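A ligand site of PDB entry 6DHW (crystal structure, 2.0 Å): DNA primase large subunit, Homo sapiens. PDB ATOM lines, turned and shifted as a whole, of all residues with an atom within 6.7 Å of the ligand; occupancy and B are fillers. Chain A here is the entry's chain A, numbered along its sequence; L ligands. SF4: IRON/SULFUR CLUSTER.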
ATOM      1  N   PRO A  20      23.225  13.427  -6.270  1.00  0.00           N
ATOM      2  CA  PRO A  20      22.197  13.374  -7.314  1.00  0.00           C
ATOM      3  C   PRO A  20      22.812  12.976  -8.647  1.00  0.00           C
ATOM      4  O   PRO A  20      24.035  13.073  -8.824  1.00  0.00           O
ATOM      5  CB  PRO A  20      21.663  14.813  -7.356  1.00  0.00           C
ATOM      6  CG  PRO A  20      22.787  15.642  -6.866  1.00  0.00           C
ATOM      7  CD  PRO A  20      23.504  14.800  -5.831  1.00  0.00           C
ATOM      8  N   PRO A  21      21.994  12.504  -9.600  1.00  0.00           N
ATOM      9  CA  PRO A  21      22.565  12.036 -10.871  1.00  0.00           C
ATOM     10  C   PRO A  21      23.453  13.048 -11.565  1.00  0.00           C
ATOM     11  O   PRO A  21      24.463  12.657 -12.173  1.00  0.00           O
ATOM     12  CB  PRO A  21      21.313  11.709 -11.698  1.00  0.00           C
ATOM     13  CG  PRO A  21      20.292  11.330 -10.668  1.00  0.00           C
ATOM     14  CD  PRO A  21      20.549  12.254  -9.510  1.00  0.00           C
ATOM     15  N   CYS A  22      23.133  14.346 -11.461  1.00  0.00           N
ATOM     16  CA  CYS A  22      23.932  15.358 -12.131  1.00  0.00           C
ATOM     17  C   CYS A  22      25.347  15.386 -11.603  1.00  0.00           C
ATOM     18  O   CYS A  22      26.302  15.564 -12.375  1.00  0.00           O
ATOM     19  CB  CYS A  22      23.286  16.737 -11.980  1.00  0.00           C
ATOM     20  SG  CYS A  22      23.246  17.310 -10.279  1.00  0.00           S
ATOM     21  N   MET A  23      25.525  15.210 -10.286  1.00  0.00           N
ATOM     22  CA  MET A  23      26.851  15.216  -9.687  1.00  0.00           C
ATOM     23  C   MET A  23      27.503  13.840  -9.726  1.00  0.00           C
ATOM     24  O   MET A  23      28.742  13.754  -9.805  1.00  0.00           O
ATOM     25  CB  MET A  23      26.763  15.693  -8.241  1.00  0.00           C
ATOM     26  CG  MET A  23      26.093  17.044  -8.084  1.00  0.00           C
ATOM     27  SD  MET A  23      26.860  18.319  -9.108  1.00  0.00           S
ATOM     28  CE  MET A  23      25.662  19.656  -8.930  1.00  0.00           C
ATOM     29  N   GLN A  43      30.163  23.149 -12.086  1.00  0.00           N
ATOM     30  CA  GLN A  43      29.014  22.485 -11.489  1.00  0.00           C
ATOM     31  C   GLN A  43      29.432  21.535 -10.375  1.00  0.00           C
ATOM     32  O   GLN A  43      28.903  21.589  -9.256  1.00  0.00           O
ATOM     33  CB  GLN A  43      28.211  21.747 -12.564  1.00  0.00           C
ATOM     34  CG  GLN A  43      26.984  21.015 -12.032  1.00  0.00           C
ATOM     35  CD  GLN A  43      26.074  20.510 -13.138  1.00  0.00           C
ATOM     36  OE1 GLN A  43      25.984  21.109 -14.206  1.00  0.00           O
ATOM     37  NE2 GLN A  43      25.408  19.395 -12.883  1.00  0.00           N
ATOM     38  N   SER A 101      21.801  25.774  -8.360  1.00  0.00           N
ATOM     39  CA  SER A 101      20.507  25.189  -8.059  1.00  0.00           C
ATOM     40  C   SER A 101      20.057  24.274  -9.201  1.00  0.00           C
ATOM     41  O   SER A 101      20.680  24.218 -10.269  1.00  0.00           O
ATOM     42  CB  SER A 101      19.470  26.296  -7.826  1.00  0.00           C
ATOM     43  OG  SER A 101      19.132  26.928  -9.056  1.00  0.00           O
ATOM     44  N   CYS A 102      18.968  23.546  -8.966  1.00  0.00           N
ATOM     45  CA  CYS A 102      18.410  22.697 -10.008  1.00  0.00           C
ATOM     46  C   CYS A 102      17.995  23.513 -11.217  1.00  0.00           C
ATOM     47  O   CYS A 102      18.248  23.133 -12.359  1.00  0.00           O
ATOM     48  CB  CYS A 102      17.213  21.908  -9.481  1.00  0.00           C
ATOM     49  SG  CYS A 102      17.617  20.739  -8.214  1.00  0.00           S
ATOM     50  N   LEU A 103      17.311  24.632 -10.978  1.00  0.00           N
ATOM     51  CA  LEU A 103      16.816  25.424 -12.093  1.00  0.00           C
ATOM     52  C   LEU A 103      17.949  26.050 -12.894  1.00  0.00           C
ATOM     53  O   LEU A 103      17.843  26.177 -14.116  1.00  0.00           O
ATOM     54  CB  LEU A 103      15.845  26.492 -11.585  1.00  0.00           C
ATOM     55  CG  LEU A 103      14.400  26.017 -11.440  1.00  0.00           C
ATOM     56  CD1 LEU A 103      13.476  27.173 -11.108  1.00  0.00           C
ATOM     57  CD2 LEU A 103      13.931  25.275 -12.684  1.00  0.00           C
ATOM     58  N   ILE A 105      20.933  24.641 -13.311  1.00  0.00           N
ATOM     59  CA  ILE A 105      21.503  23.544 -14.070  1.00  0.00           C
ATOM     60  C   ILE A 105      20.602  23.177 -15.252  1.00  0.00           C
ATOM     61  O   ILE A 105      21.074  22.934 -16.370  1.00  0.00           O
ATOM     62  CB  ILE A 105      21.750  22.341 -13.146  1.00  0.00           C
ATOM     63  CG1 ILE A 105      22.847  22.660 -12.126  1.00  0.00           C
ATOM     64  CG2 ILE A 105      22.122  21.102 -13.938  1.00  0.00           C
ATOM     65  CD1 ILE A 105      23.008  21.609 -11.053  1.00  0.00           C
ATOM     66  N   ILE A 106      19.296  23.148 -15.024  1.00  0.00           N
ATOM     67  CA  ILE A 106      18.361  22.697 -16.049  1.00  0.00           C
ATOM     68  C   ILE A 106      18.184  23.760 -17.132  1.00  0.00           C
ATOM     69  O   ILE A 106      18.170  23.436 -18.322  1.00  0.00           O
ATOM     70  CB  ILE A 106      17.008  22.331 -15.392  1.00  0.00           C
ATOM     71  CG1 ILE A 106      17.128  20.976 -14.687  1.00  0.00           C
ATOM     72  CG2 ILE A 106      15.893  22.330 -16.425  1.00  0.00           C
ATOM     73  CD1 ILE A 106      16.026  20.711 -13.684  1.00  0.00           C
ATOM     74  N   GLY A 118      25.310  19.505 -16.485  1.00  0.00           N
ATOM     75  CA  GLY A 118      23.887  19.542 -16.771  1.00  0.00           C
ATOM     76  C   GLY A 118      23.091  18.593 -15.890  1.00  0.00           C
ATOM     77  O   GLY A 118      23.584  18.038 -14.902  1.00  0.00           O
ATOM     78  N   CYS A 119      21.828  18.431 -16.262  1.00  0.00           N
ATOM     79  CA  CYS A 119      20.907  17.576 -15.525  1.00  0.00           C
ATOM     80  C   CYS A 119      20.516  16.397 -16.406  1.00  0.00           C
ATOM     81  O   CYS A 119      19.929  16.614 -17.469  1.00  0.00           O
ATOM     82  CB  CYS A 119      19.678  18.356 -15.087  1.00  0.00           C
ATOM     83  SG  CYS A 119      18.260  17.342 -14.619  1.00  0.00           S
ATOM     84  N   PRO A 120      20.848  15.169 -16.021  1.00  0.00           N
ATOM     85  CA  PRO A 120      20.567  14.017 -16.900  1.00  0.00           C
ATOM     86  C   PRO A 120      19.097  13.879 -17.275  1.00  0.00           C
ATOM     87  O   PRO A 120      18.798  13.456 -18.391  1.00  0.00           O
ATOM     88  CB  PRO A 120      21.048  12.816 -16.077  1.00  0.00           C
ATOM     89  CG  PRO A 120      21.975  13.378 -15.055  1.00  0.00           C
ATOM     90  CD  PRO A 120      21.507  14.762 -14.764  1.00  0.00           C
ATOM     91  N   PHE A 121      18.185  14.234 -16.375  1.00  0.00           N
ATOM     92  CA  PHE A 121      16.764  14.116 -16.709  1.00  0.00           C
ATOM     93  C   PHE A 121      16.354  15.088 -17.802  1.00  0.00           C
ATOM     94  O   PHE A 121      15.503  14.758 -18.631  1.00  0.00           O
ATOM     95  CB  PHE A 121      15.926  14.333 -15.452  1.00  0.00           C
ATOM     96  CG  PHE A 121      16.243  13.372 -14.354  1.00  0.00           C
ATOM     97  CD1 PHE A 121      15.826  12.057 -14.429  1.00  0.00           C
ATOM     98  CD2 PHE A 121      16.968  13.774 -13.251  1.00  0.00           C
ATOM     99  CE1 PHE A 121      16.132  11.164 -13.416  1.00  0.00           C
ATOM    100  CE2 PHE A 121      17.278  12.890 -12.234  1.00  0.00           C
ATOM    101  CZ  PHE A 121      16.854  11.583 -12.319  1.00  0.00           C
ATOM    102  N   ARG A 122      16.962  16.273 -17.834  1.00  0.00           N
ATOM    103  CA  ARG A 122      16.680  17.277 -18.854  1.00  0.00           C
ATOM    104  C   ARG A 122      17.555  17.123 -20.100  1.00  0.00           C
ATOM    105  O   ARG A 122      17.078  17.335 -21.217  1.00  0.00           O
ATOM    106  CB  ARG A 122      16.843  18.678 -18.254  1.00  0.00           C
ATOM    107  CG  ARG A 122      17.180  19.787 -19.239  1.00  0.00           C
ATOM    108  CD  ARG A 122      15.968  20.201 -20.078  1.00  0.00           C
ATOM    109  NE  ARG A 122      16.308  21.278 -20.998  1.00  0.00           N
ATOM    110  CZ  ARG A 122      16.887  21.097 -22.189  1.00  0.00           C
ATOM    111  NH1 ARG A 122      17.166  19.869 -22.603  1.00  0.00           N
ATOM    112  NH2 ARG A 122      17.160  22.137 -22.953  1.00  0.00           N
ATOM    113  N   TYR A 155      11.453  17.252 -14.361  1.00  0.00           N
ATOM    114  CA  TYR A 155      12.792  16.722 -14.130  1.00  0.00           C
ATOM    115  C   TYR A 155      13.073  16.531 -12.643  1.00  0.00           C
ATOM    116  O   TYR A 155      13.561  15.472 -12.224  1.00  0.00           O
ATOM    117  CB  TYR A 155      13.821  17.664 -14.766  1.00  0.00           C
ATOM    118  CG  TYR A 155      13.512  17.976 -16.212  1.00  0.00           C
ATOM    119  CD1 TYR A 155      13.467  16.963 -17.161  1.00  0.00           C
ATOM    120  CD2 TYR A 155      13.234  19.277 -16.623  1.00  0.00           C
ATOM    121  CE1 TYR A 155      13.169  17.238 -18.488  1.00  0.00           C
ATOM    122  CE2 TYR A 155      12.940  19.561 -17.946  1.00  0.00           C
ATOM    123  CZ  TYR A 155      12.912  18.542 -18.872  1.00  0.00           C
ATOM    124  OH  TYR A 155      12.615  18.822 -20.185  1.00  0.00           O
ATOM    125  N   GLN A 156      12.740  17.531 -11.826  1.00  0.00           N
ATOM    126  CA  GLN A 156      13.013  17.442 -10.400  1.00  0.00           C
ATOM    127  C   GLN A 156      12.134  16.396  -9.717  1.00  0.00           C
ATOM    128  O   GLN A 156      12.576  15.739  -8.769  1.00  0.00           O
ATOM    129  CB  GLN A 156      12.838  18.818  -9.763  1.00  0.00           C
ATOM    130  CG  GLN A 156      13.878  19.806 -10.259  1.00  0.00           C
ATOM    131  CD  GLN A 156      13.411  21.242 -10.177  1.00  0.00           C
ATOM    132  OE1 GLN A 156      13.111  21.865 -11.195  1.00  0.00           O
ATOM    133  NE2 GLN A 156      13.352  21.783  -8.963  1.00  0.00           N
ATOM    134  N   VAL A 157      10.897  16.203 -10.193  1.00  0.00           N
ATOM    135  CA  VAL A 157      10.074  15.147  -9.633  1.00  0.00           C
ATOM    136  C   VAL A 157      10.640  13.780  -9.994  1.00  0.00           C
ATOM    137  O   VAL A 157      10.635  12.844  -9.176  1.00  0.00           O
ATOM    138  CB  VAL A 157       8.613  15.301 -10.112  1.00  0.00           C
ATOM    139  CG1 VAL A 157       7.735  14.221  -9.508  1.00  0.00           C
ATOM    140  CG2 VAL A 157       8.085  16.681  -9.738  1.00  0.00           C
ATOM    141  N   ALA A 158      11.138  13.637 -11.221  1.00  0.00           N
ATOM    142  CA  ALA A 158      11.829  12.411 -11.610  1.00  0.00           C
ATOM    143  C   ALA A 158      13.043  12.163 -10.729  1.00  0.00           C
ATOM    144  O   ALA A 158      13.343  11.009 -10.376  1.00  0.00           O
ATOM    145  CB  ALA A 158      12.225  12.482 -13.082  1.00  0.00           C
ATOM    146  N   CYS A 159      13.762  13.224 -10.369  1.00  0.00           N
ATOM    147  CA  CYS A 159      14.908  13.049  -9.485  1.00  0.00           C
ATOM    148  C   CYS A 159      14.474  12.670  -8.074  1.00  0.00           C
ATOM    149  O   CYS A 159      15.168  11.907  -7.386  1.00  0.00           O
ATOM    150  CB  CYS A 159      15.772  14.308  -9.465  1.00  0.00           C
ATOM    151  SG  CYS A 159      17.336  14.007  -8.637  1.00  0.00           S
ATOM    152  N   GLN A 160      13.350  13.213  -7.596  1.00  0.00           N
ATOM    153  CA  GLN A 160      12.809  12.771  -6.310  1.00  0.00           C
ATOM    154  C   GLN A 160      12.470  11.283  -6.357  1.00  0.00           C
ATOM    155  O   GLN A 160      12.664  10.557  -5.381  1.00  0.00           O
ATOM    156  CB  GLN A 160      11.574  13.603  -5.951  1.00  0.00           C
ATOM    157  CG  GLN A 160      11.879  15.032  -5.529  1.00  0.00           C
ATOM    158  CD  GLN A 160      10.621  15.849  -5.269  1.00  0.00           C
ATOM    159  OE1 GLN A 160      10.687  17.065  -5.090  1.00  0.00           O
ATOM    160  NE2 GLN A 160       9.467  15.172  -5.237  1.00  0.00           N
ATOM    161  N   LEU A 176      12.356  18.941  -3.988  1.00  0.00           N
ATOM    162  CA  LEU A 176      13.722  19.053  -4.467  1.00  0.00           C
ATOM    163  C   LEU A 176      13.888  20.320  -5.297  1.00  0.00           C
ATOM    164  O   LEU A 176      13.184  20.526  -6.291  1.00  0.00           O
ATOM    165  CB  LEU A 176      14.113  17.829  -5.281  1.00  0.00           C
ATOM    166  CG  LEU A 176      15.445  17.981  -6.014  1.00  0.00           C
ATOM    167  CD1 LEU A 176      16.594  18.058  -5.022  1.00  0.00           C
ATOM    168  CD2 LEU A 176      15.652  16.841  -7.001  1.00  0.00           C
ATOM    169  N   ASN A 177      14.832  21.177  -4.890  1.00  0.00           N
ATOM    170  CA  ASN A 177      15.209  22.327  -5.698  1.00  0.00           C
ATOM    171  C   ASN A 177      16.716  22.601  -5.743  1.00  0.00           C
ATOM    172  O   ASN A 177      17.119  23.611  -6.326  1.00  0.00           O
ATOM    173  CB  ASN A 177      14.475  23.573  -5.168  1.00  0.00           C
ATOM    174  CG  ASN A 177      14.883  23.937  -3.745  1.00  0.00           C
ATOM    175  OD1 ASN A 177      16.014  24.338  -3.496  1.00  0.00           O
ATOM    176  ND2 ASN A 177      13.958  23.774  -2.807  1.00  0.00           N
ATOM    177  N   HIS A 178      17.552  21.718  -5.191  1.00  0.00           N
ATOM    178  CA  HIS A 178      18.982  21.970  -5.174  1.00  0.00           C
ATOM    179  C   HIS A 178      19.767  20.680  -5.009  1.00  0.00           C
ATOM    180  O   HIS A 178      19.425  19.849  -4.158  1.00  0.00           O
ATOM    181  CB  HIS A 178      19.334  22.959  -4.058  1.00  0.00           C
ATOM    182  CG  HIS A 178      20.618  23.689  -4.260  1.00  0.00           C
ATOM    183  ND1 HIS A 178      21.854  23.074  -4.184  1.00  0.00           N
ATOM    184  CD2 HIS A 178      20.874  24.985  -4.556  1.00  0.00           C
ATOM    185  CE1 HIS A 178      22.803  23.959  -4.410  1.00  0.00           C
ATOM    186  NE2 HIS A 178      22.240  25.123  -4.642  1.00  0.00           N
ATOM    187  N   PRO A 179      20.814  20.453  -5.819  1.00  0.00           N
ATOM    188  CA  PRO A 179      21.632  19.243  -5.627  1.00  0.00           C
ATOM    189  C   PRO A 179      22.171  19.089  -4.212  1.00  0.00           C
ATOM    190  O   PRO A 179      22.213  17.966  -3.685  1.00  0.00           O
ATOM    191  CB  PRO A 179      22.772  19.441  -6.647  1.00  0.00           C
ATOM    192  CG  PRO A 179      22.175  20.308  -7.711  1.00  0.00           C
ATOM    193  CD  PRO A 179      21.268  21.250  -6.965  1.00  0.00           C
ATOM    194  N   ASN A 180      22.585  20.187  -3.576  1.00  0.00           N
ATOM    195  CA  ASN A 180      23.103  20.079  -2.213  1.00  0.00           C
ATOM    196  C   ASN A 180      21.996  19.748  -1.215  1.00  0.00           C
ATOM    197  O   ASN A 180      22.254  19.104  -0.193  1.00  0.00           O
ATOM    198  CB  ASN A 180      23.811  21.379  -1.828  1.00  0.00           C
ATOM    199  CG  ASN A 180      25.139  21.549  -2.544  1.00  0.00           C
ATOM    200  OD1 ASN A 180      25.214  22.181  -3.596  1.00  0.00           O
ATOM    201  ND2 ASN A 180      26.198  20.965  -1.991  1.00  0.00           N
ATOM    202  N   PHE A 182      19.503  17.704  -2.070  1.00  0.00           N
ATOM    203  CA  PHE A 182      19.511  16.269  -2.295  1.00  0.00           C
ATOM    204  C   PHE A 182      20.555  15.587  -1.422  1.00  0.00           C
ATOM    205  O   PHE A 182      20.263  14.594  -0.743  1.00  0.00           O
ATOM    206  CB  PHE A 182      19.777  16.001  -3.786  1.00  0.00           C
ATOM    207  CG  PHE A 182      19.628  14.555  -4.203  1.00  0.00           C
ATOM    208  CD1 PHE A 182      20.551  13.597  -3.813  1.00  0.00           C
ATOM    209  CD2 PHE A 182      18.591  14.171  -5.038  1.00  0.00           C
ATOM    210  CE1 PHE A 182      20.422  12.279  -4.220  1.00  0.00           C
ATOM    211  CE2 PHE A 182      18.456  12.860  -5.454  1.00  0.00           C
ATOM    212  CZ  PHE A 182      19.372  11.916  -5.039  1.00  0.00           C
HETATM  213 FE1  SF4 L   1      20.696  17.445 -10.282  1.00  0.00          FE
HETATM  214 FE2  SF4 L   1      18.672  17.374 -12.076  1.00  0.00          FE
HETATM  215 FE3  SF4 L   1      18.403  18.805  -9.765  1.00  0.00          FE
HETATM  216 FE4  SF4 L   1      18.410  16.089  -9.687  1.00  0.00          FE
HETATM  217  S1  SF4 L   1      16.863  17.413 -10.706  1.00  0.00           S
HETATM  218  S2  SF4 L   1      19.560  17.488  -8.314  1.00  0.00           S
HETATM  219  S3  SF4 L   1      19.898  15.607 -11.342  1.00  0.00           S
HETATM  220  S4  SF4 L   1      19.862  19.208 -11.456  1.00  0.00           S
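The backbone NH of Cys 22 sits close to a sulfur (S3) of the ligand (3.5 Å).
FE1 of the ligand is bound by SG of Cys 22, 2.6 Å away.
An iron atom (FE4) of the ligand is bound by the side-chain sulfur of Cys 159.
An iron atom (FE2) of the ligand is bound by the side-chain sulfur of Cys 119, at 2.6 Å.
SG of Cys 102 is bound to FE3 of the ligand, 2.6 Å away.
Residues that only touch the ligand: Pro 20 (3.5 Å), Pro 21 (3.9 Å), Ile 105 (3.9 Å), Pro 120 (3.9 Å), Phe 121 (3.9 Å), Gln 156 (3.9 Å), Leu 176 (3.9 Å) and Pro 179 (3.8 Å).
Hydrophobic or aromatic side chains that line the ligand: Pro 20, Pro 21, Ile 105, Pro 120, Phe 121, Leu 176 and Pro 179.
Along chain A the residues within 4 Å of the ligand span positions 20 to 179.
The nearest printed residue that does not touch the ligand is Tyr 155 (4.1 Å).
The side-chain sulfur (SG) of Cys 119 sits close to the backbone NH (N) of Phe 121, 3.6 Å away.
N of Arg 122 lies close to SG of Cys 119 (3.6 Å).
The side-chain sulfur (SG) of Cys 102 lies close to the backbone NH (N) of His 178, at 3.2 Å.
The backbone NH (N) of Cys 102 is in hydrogen-bond range of the backbone carbonyl oxygen (O) of Asn 177 (3.2 Å).
The side-chain amide nitrogen (NE2) of Gln 156 is in hydrogen-bond range of the backbone carbonyl oxygen (O) of Leu 176 (3.0 Å).
The side-chain amide oxygen (OE1) of Gln 160 lies within hydrogen-bond range of the backbone NH (N) of Leu 176, at 2.7 Å.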
